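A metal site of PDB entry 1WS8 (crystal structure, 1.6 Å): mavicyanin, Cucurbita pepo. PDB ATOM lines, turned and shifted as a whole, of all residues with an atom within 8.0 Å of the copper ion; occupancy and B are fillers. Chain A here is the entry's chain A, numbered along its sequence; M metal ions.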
ATOM      1  N   TRP A  13      -7.124  23.833 -19.282  1.00  0.00           N
ATOM      2  CA  TRP A  13      -6.497  24.430 -18.097  1.00  0.00           C
ATOM      3  C   TRP A  13      -5.789  23.271 -17.403  1.00  0.00           C
ATOM      4  O   TRP A  13      -6.438  22.413 -16.789  1.00  0.00           O
ATOM      5  CB  TRP A  13      -7.617  25.014 -17.229  1.00  0.00           C
ATOM      6  CG  TRP A  13      -7.226  25.829 -16.028  1.00  0.00           C
ATOM      7  CD1 TRP A  13      -7.606  25.606 -14.741  1.00  0.00           C
ATOM      8  CD2 TRP A  13      -6.489  27.069 -16.019  1.00  0.00           C
ATOM      9  NE1 TRP A  13      -7.170  26.628 -13.918  1.00  0.00           N
ATOM     10  CE2 TRP A  13      -6.488  27.545 -14.682  1.00  0.00           C
ATOM     11  CE3 TRP A  13      -5.848  27.832 -17.003  1.00  0.00           C
ATOM     12  CZ2 TRP A  13      -5.867  28.742 -14.302  1.00  0.00           C
ATOM     13  CZ3 TRP A  13      -5.227  29.029 -16.622  1.00  0.00           C
ATOM     14  CH2 TRP A  13      -5.246  29.465 -15.288  1.00  0.00           C
ATOM     15  N   THR A  14      -4.464  23.241 -17.491  1.00  0.00           N
ATOM     16  CA  THR A  14      -3.705  22.112 -16.934  1.00  0.00           C
ATOM     17  C   THR A  14      -2.264  22.426 -16.549  1.00  0.00           C
ATOM     18  O   THR A  14      -1.746  23.508 -16.829  1.00  0.00           O
ATOM     19  CB  THR A  14      -3.672  20.973 -17.972  1.00  0.00           C
ATOM     20  OG1 THR A  14      -3.023  19.822 -17.410  1.00  0.00           O
ATOM     21  CG2 THR A  14      -2.901  21.418 -19.221  1.00  0.00           C
ATOM     22  N   THR A  15      -1.623  21.456 -15.898  1.00  0.00           N
ATOM     23  CA  THR A  15      -0.221  21.571 -15.521  1.00  0.00           C
ATOM     24  C   THR A  15       0.505  20.293 -15.978  1.00  0.00           C
ATOM     25  O   THR A  15       1.679  20.120 -15.684  1.00  0.00           O
ATOM     26  CB  THR A  15       0.010  21.719 -13.986  1.00  0.00           C
ATOM     27  OG1 THR A  15      -0.659  20.670 -13.275  1.00  0.00           O
ATOM     28  CG2 THR A  15      -0.500  23.080 -13.501  1.00  0.00           C
ATOM     29  N   LEU A  16      -0.200  19.423 -16.698  1.00  0.00           N
ATOM     30  CA  LEU A  16       0.394  18.165 -17.166  1.00  0.00           C
ATOM     31  C   LEU A  16       1.662  18.419 -17.969  1.00  0.00           C
ATOM     32  O   LEU A  16       2.673  17.710 -17.832  1.00  0.00           O
ATOM     33  CB  LEU A  16      -0.596  17.377 -18.029  1.00  0.00           C
ATOM     34  CG  LEU A  16      -0.733  15.881 -17.726  1.00  0.00           C
ATOM     35  CD1 LEU A  16      -1.218  15.160 -18.966  1.00  0.00           C
ATOM     36  CD2 LEU A  16       0.600  15.305 -17.294  1.00  0.00           C
ATOM     37  N   TYR A  40     -11.137  21.551 -16.990  1.00  0.00           N
ATOM     38  CA  TYR A  40     -10.067  20.886 -16.247  1.00  0.00           C
ATOM     39  C   TYR A  40     -10.611  19.803 -15.333  1.00  0.00           C
ATOM     40  O   TYR A  40     -11.824  19.673 -15.156  1.00  0.00           O
ATOM     41  CB  TYR A  40      -9.315  21.929 -15.406  1.00  0.00           C
ATOM     42  CG  TYR A  40     -10.186  22.695 -14.443  1.00  0.00           C
ATOM     43  CD1 TYR A  40     -10.388  22.255 -13.130  1.00  0.00           C
ATOM     44  CD2 TYR A  40     -10.853  23.850 -14.852  1.00  0.00           C
ATOM     45  CE1 TYR A  40     -11.230  22.944 -12.250  1.00  0.00           C
ATOM     46  CE2 TYR A  40     -11.701  24.551 -13.975  1.00  0.00           C
ATOM     47  CZ  TYR A  40     -11.876  24.095 -12.682  1.00  0.00           C
ATOM     48  OH  TYR A  40     -12.721  24.762 -11.826  1.00  0.00           O
ATOM     49  N   ASN A  41      -9.709  19.008 -14.781  1.00  0.00           N
ATOM     50  CA  ASN A  41     -10.086  17.956 -13.832  1.00  0.00           C
ATOM     51  C   ASN A  41     -10.139  18.682 -12.505  1.00  0.00           C
ATOM     52  O   ASN A  41      -9.099  19.064 -11.964  1.00  0.00           O
ATOM     53  CB  ASN A  41      -9.007  16.877 -13.795  1.00  0.00           C
ATOM     54  CG  ASN A  41      -9.366  15.738 -12.851  1.00  0.00           C
ATOM     55  OD1 ASN A  41     -10.033  15.940 -11.849  1.00  0.00           O
ATOM     56  ND2 ASN A  41      -8.898  14.535 -13.183  1.00  0.00           N
ATOM     57  N   PHE A  44      -7.724  18.233  -9.479  1.00  0.00           N
ATOM     58  CA  PHE A  44      -6.358  18.751  -9.508  1.00  0.00           C
ATOM     59  C   PHE A  44      -6.224  20.265  -9.620  1.00  0.00           C
ATOM     60  O   PHE A  44      -5.179  20.818  -9.277  1.00  0.00           O
ATOM     61  CB  PHE A  44      -5.582  18.139 -10.684  1.00  0.00           C
ATOM     62  CG  PHE A  44      -5.269  16.679 -10.513  1.00  0.00           C
ATOM     63  CD1 PHE A  44      -6.219  15.714 -10.810  1.00  0.00           C
ATOM     64  CD2 PHE A  44      -4.013  16.287 -10.057  1.00  0.00           C
ATOM     65  CE1 PHE A  44      -5.921  14.356 -10.644  1.00  0.00           C
ATOM     66  CE2 PHE A  44      -3.715  14.929  -9.892  1.00  0.00           C
ATOM     67  CZ  PHE A  44      -4.670  13.977 -10.192  1.00  0.00           C
ATOM     68  N   HIS A  45      -7.265  20.939 -10.103  1.00  0.00           N
ATOM     69  CA  HIS A  45      -7.172  22.385 -10.300  1.00  0.00           C
ATOM     70  C   HIS A  45      -8.440  23.144  -9.939  1.00  0.00           C
ATOM     71  O   HIS A  45      -9.487  22.560  -9.659  1.00  0.00           O
ATOM     72  CB  HIS A  45      -6.891  22.688 -11.778  1.00  0.00           C
ATOM     73  CG  HIS A  45      -5.772  21.885 -12.360  1.00  0.00           C
ATOM     74  ND1 HIS A  45      -4.446  22.160 -12.108  1.00  0.00           N
ATOM     75  CD2 HIS A  45      -5.782  20.796 -13.167  1.00  0.00           C
ATOM     76  CE1 HIS A  45      -3.686  21.274 -12.731  1.00  0.00           C
ATOM     77  NE2 HIS A  45      -4.473  20.440 -13.382  1.00  0.00           N
ATOM     78  N   ASN A  46      -8.319  24.470  -9.961  1.00  0.00           N
ATOM     79  CA  ASN A  46      -9.437  25.369  -9.715  1.00  0.00           C
ATOM     80  C   ASN A  46      -9.113  26.670 -10.435  1.00  0.00           C
ATOM     81  O   ASN A  46      -8.059  26.792 -11.073  1.00  0.00           O
ATOM     82  CB  ASN A  46      -9.703  25.580  -8.217  1.00  0.00           C
ATOM     83  CG  ASN A  46      -8.566  26.269  -7.474  1.00  0.00           C
ATOM     84  OD1 ASN A  46      -8.492  26.180  -6.240  1.00  0.00           O
ATOM     85  ND2 ASN A  46      -7.699  26.970  -8.189  1.00  0.00           N
ATOM     86  N   VAL A  47     -10.026  27.628 -10.385  1.00  0.00           N
ATOM     87  CA  VAL A  47      -9.805  28.914 -11.044  1.00  0.00           C
ATOM     88  C   VAL A  47     -10.117  29.994 -10.021  1.00  0.00           C
ATOM     89  O   VAL A  47     -11.202  30.000  -9.448  1.00  0.00           O
ATOM     90  CB  VAL A  47     -10.729  29.109 -12.265  1.00  0.00           C
ATOM     91  CG1 VAL A  47     -10.471  30.470 -12.905  1.00  0.00           C
ATOM     92  CG2 VAL A  47     -10.508  27.992 -13.280  1.00  0.00           C
ATOM     93  N   LEU A  85      -5.870  32.591 -11.882  1.00  0.00           N
ATOM     94  CA  LEU A  85      -4.786  31.653 -11.610  1.00  0.00           C
ATOM     95  C   LEU A  85      -5.328  30.437 -10.873  1.00  0.00           C
ATOM     96  O   LEU A  85      -6.408  30.485 -10.298  1.00  0.00           O
ATOM     97  CB  LEU A  85      -3.669  32.313 -10.789  1.00  0.00           C
ATOM     98  CG  LEU A  85      -3.990  32.956  -9.425  1.00  0.00           C
ATOM     99  CD1 LEU A  85      -4.285  31.898  -8.380  1.00  0.00           C
ATOM    100  CD2 LEU A  85      -2.803  33.793  -8.993  1.00  0.00           C
ATOM    101  N   CYS A  86      -4.575  29.347 -10.929  1.00  0.00           N
ATOM    102  CA  CYS A  86      -4.972  28.138 -10.223  1.00  0.00           C
ATOM    103  C   CYS A  86      -4.345  28.278  -8.834  1.00  0.00           C
ATOM    104  O   CYS A  86      -3.156  28.564  -8.727  1.00  0.00           O
ATOM    105  CB  CYS A  86      -4.427  26.893 -10.918  1.00  0.00           C
ATOM    106  SG  CYS A  86      -4.775  25.405  -9.978  1.00  0.00           S
ATOM    107  N   GLY A  87      -5.149  28.087  -7.790  1.00  0.00           N
ATOM    108  CA  GLY A  87      -4.662  28.238  -6.439  1.00  0.00           C
ATOM    109  C   GLY A  87      -4.032  27.024  -5.774  1.00  0.00           C
ATOM    110  O   GLY A  87      -3.543  27.140  -4.652  1.00  0.00           O
ATOM    111  N   ILE A  88      -4.054  25.876  -6.438  1.00  0.00           N
ATOM    112  CA  ILE A  88      -3.455  24.678  -5.853  1.00  0.00           C
ATOM    113  C   ILE A  88      -1.961  24.949  -5.719  1.00  0.00           C
ATOM    114  O   ILE A  88      -1.324  25.423  -6.661  1.00  0.00           O
ATOM    115  CB  ILE A  88      -3.701  23.445  -6.746  1.00  0.00           C
ATOM    116  CG1 ILE A  88      -5.201  23.264  -6.989  1.00  0.00           C
ATOM    117  CG2 ILE A  88      -3.102  22.207  -6.093  1.00  0.00           C
ATOM    118  CD1 ILE A  88      -6.028  23.168  -5.724  1.00  0.00           C
ATOM    119  N   PRO A  89      -1.383  24.670  -4.537  1.00  0.00           N
ATOM    120  CA  PRO A  89       0.037  24.899  -4.281  1.00  0.00           C
ATOM    121  C   PRO A  89       0.986  24.585  -5.436  1.00  0.00           C
ATOM    122  O   PRO A  89       0.993  23.464  -5.963  1.00  0.00           O
ATOM    123  CB  PRO A  89       0.309  24.019  -3.064  1.00  0.00           C
ATOM    124  CG  PRO A  89      -0.976  24.123  -2.306  1.00  0.00           C
ATOM    125  CD  PRO A  89      -2.007  23.954  -3.410  1.00  0.00           C
ATOM    126  N   GLY A  90       1.761  25.586  -5.828  1.00  0.00           N
ATOM    127  CA  GLY A  90       2.735  25.429  -6.893  1.00  0.00           C
ATOM    128  C   GLY A  90       2.266  25.509  -8.332  1.00  0.00           C
ATOM    129  O   GLY A  90       3.084  25.619  -9.239  1.00  0.00           O
ATOM    130  N   HIS A  91       0.956  25.474  -8.561  1.00  0.00           N
ATOM    131  CA  HIS A  91       0.467  25.520  -9.939  1.00  0.00           C
ATOM    132  C   HIS A  91       0.652  26.855 -10.626  1.00  0.00           C
ATOM    133  O   HIS A  91       0.991  26.896 -11.807  1.00  0.00           O
ATOM    134  CB  HIS A  91      -1.004  25.103  -9.992  1.00  0.00           C
ATOM    135  CG  HIS A  91      -1.222  23.653  -9.646  1.00  0.00           C
ATOM    136  ND1 HIS A  91      -2.327  22.951 -10.085  1.00  0.00           N
ATOM    137  CD2 HIS A  91      -0.499  22.796  -8.896  1.00  0.00           C
ATOM    138  CE1 HIS A  91      -2.265  21.711  -9.615  1.00  0.00           C
ATOM    139  NE2 HIS A  91      -1.167  21.595  -8.891  1.00  0.00           N
ATOM    140  N   CYS A  92       0.443  27.941  -9.906  1.00  0.00           N
ATOM    141  CA  CYS A  92       0.609  29.268 -10.491  1.00  0.00           C
ATOM    142  C   CYS A  92       2.064  29.455 -10.900  1.00  0.00           C
ATOM    143  O   CYS A  92       2.352  30.011 -11.967  1.00  0.00           O
ATOM    144  CB  CYS A  92       0.195  30.328  -9.470  1.00  0.00           C
ATOM    145  SG  CYS A  92       0.356  32.062 -10.010  1.00  0.00           S
ATOM    146  N   LEU A  94       4.018  27.233 -11.866  1.00  0.00           N
ATOM    147  CA  LEU A  94       4.287  26.398 -13.044  1.00  0.00           C
ATOM    148  C   LEU A  94       3.755  27.083 -14.294  1.00  0.00           C
ATOM    149  O   LEU A  94       3.915  26.579 -15.399  1.00  0.00           O
ATOM    150  CB  LEU A  94       3.648  25.019 -12.880  1.00  0.00           C
ATOM    151  CG  LEU A  94       4.345  24.056 -11.922  1.00  0.00           C
ATOM    152  CD1 LEU A  94       3.554  22.758 -11.806  1.00  0.00           C
ATOM    153  CD2 LEU A  94       5.749  23.764 -12.448  1.00  0.00           C
ATOM    154  N   GLN A  96       0.349  28.264 -14.579  1.00  0.00           N
ATOM    155  CA  GLN A  96      -1.087  28.147 -14.760  1.00  0.00           C
ATOM    156  C   GLN A  96      -1.759  29.415 -14.241  1.00  0.00           C
ATOM    157  O   GLN A  96      -2.300  29.451 -13.137  1.00  0.00           O
ATOM    158  CB  GLN A  96      -1.617  26.911 -14.030  1.00  0.00           C
ATOM    159  CG  GLN A  96      -2.981  26.457 -14.519  1.00  0.00           C
ATOM    160  CD  GLN A  96      -3.475  25.218 -13.795  1.00  0.00           C
ATOM    161  OE1 GLN A  96      -3.025  24.922 -12.692  1.00  0.00           O
ATOM    162  NE2 GLN A  96      -4.419  24.506 -14.409  1.00  0.00           N
HETATM  163 CU    CU M   1      -3.854  23.770 -11.093  1.00  0.00          CU
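The side-chain sulfur of Cys 86 sits close to the backbone NH of Ile 88 (3.6 Å). The side-chain sulfur (SG) of Cys 86 lies close to the backbone NH (N) of Asn 46, at 3.7 Å. NE2 of Gln 96 sits close to N of Thr 14, at 3.3 Å.
Merely in contact with the copper ion: Phe 44 (3.7 Å). Along chain A the residues within 4 Å of the copper ion span positions 44 to 96.
The copper ion is bound by a ring nitrogen (ND1) of His 45 (2.0 Å), a ring nitrogen (ND1) of His 91 (2.0 Å), the side-chain amide oxygen (OE1) of Gln 96 (2.1 Å) and the side-chain sulfur (SG) of Cys 86 (2.2 Å).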
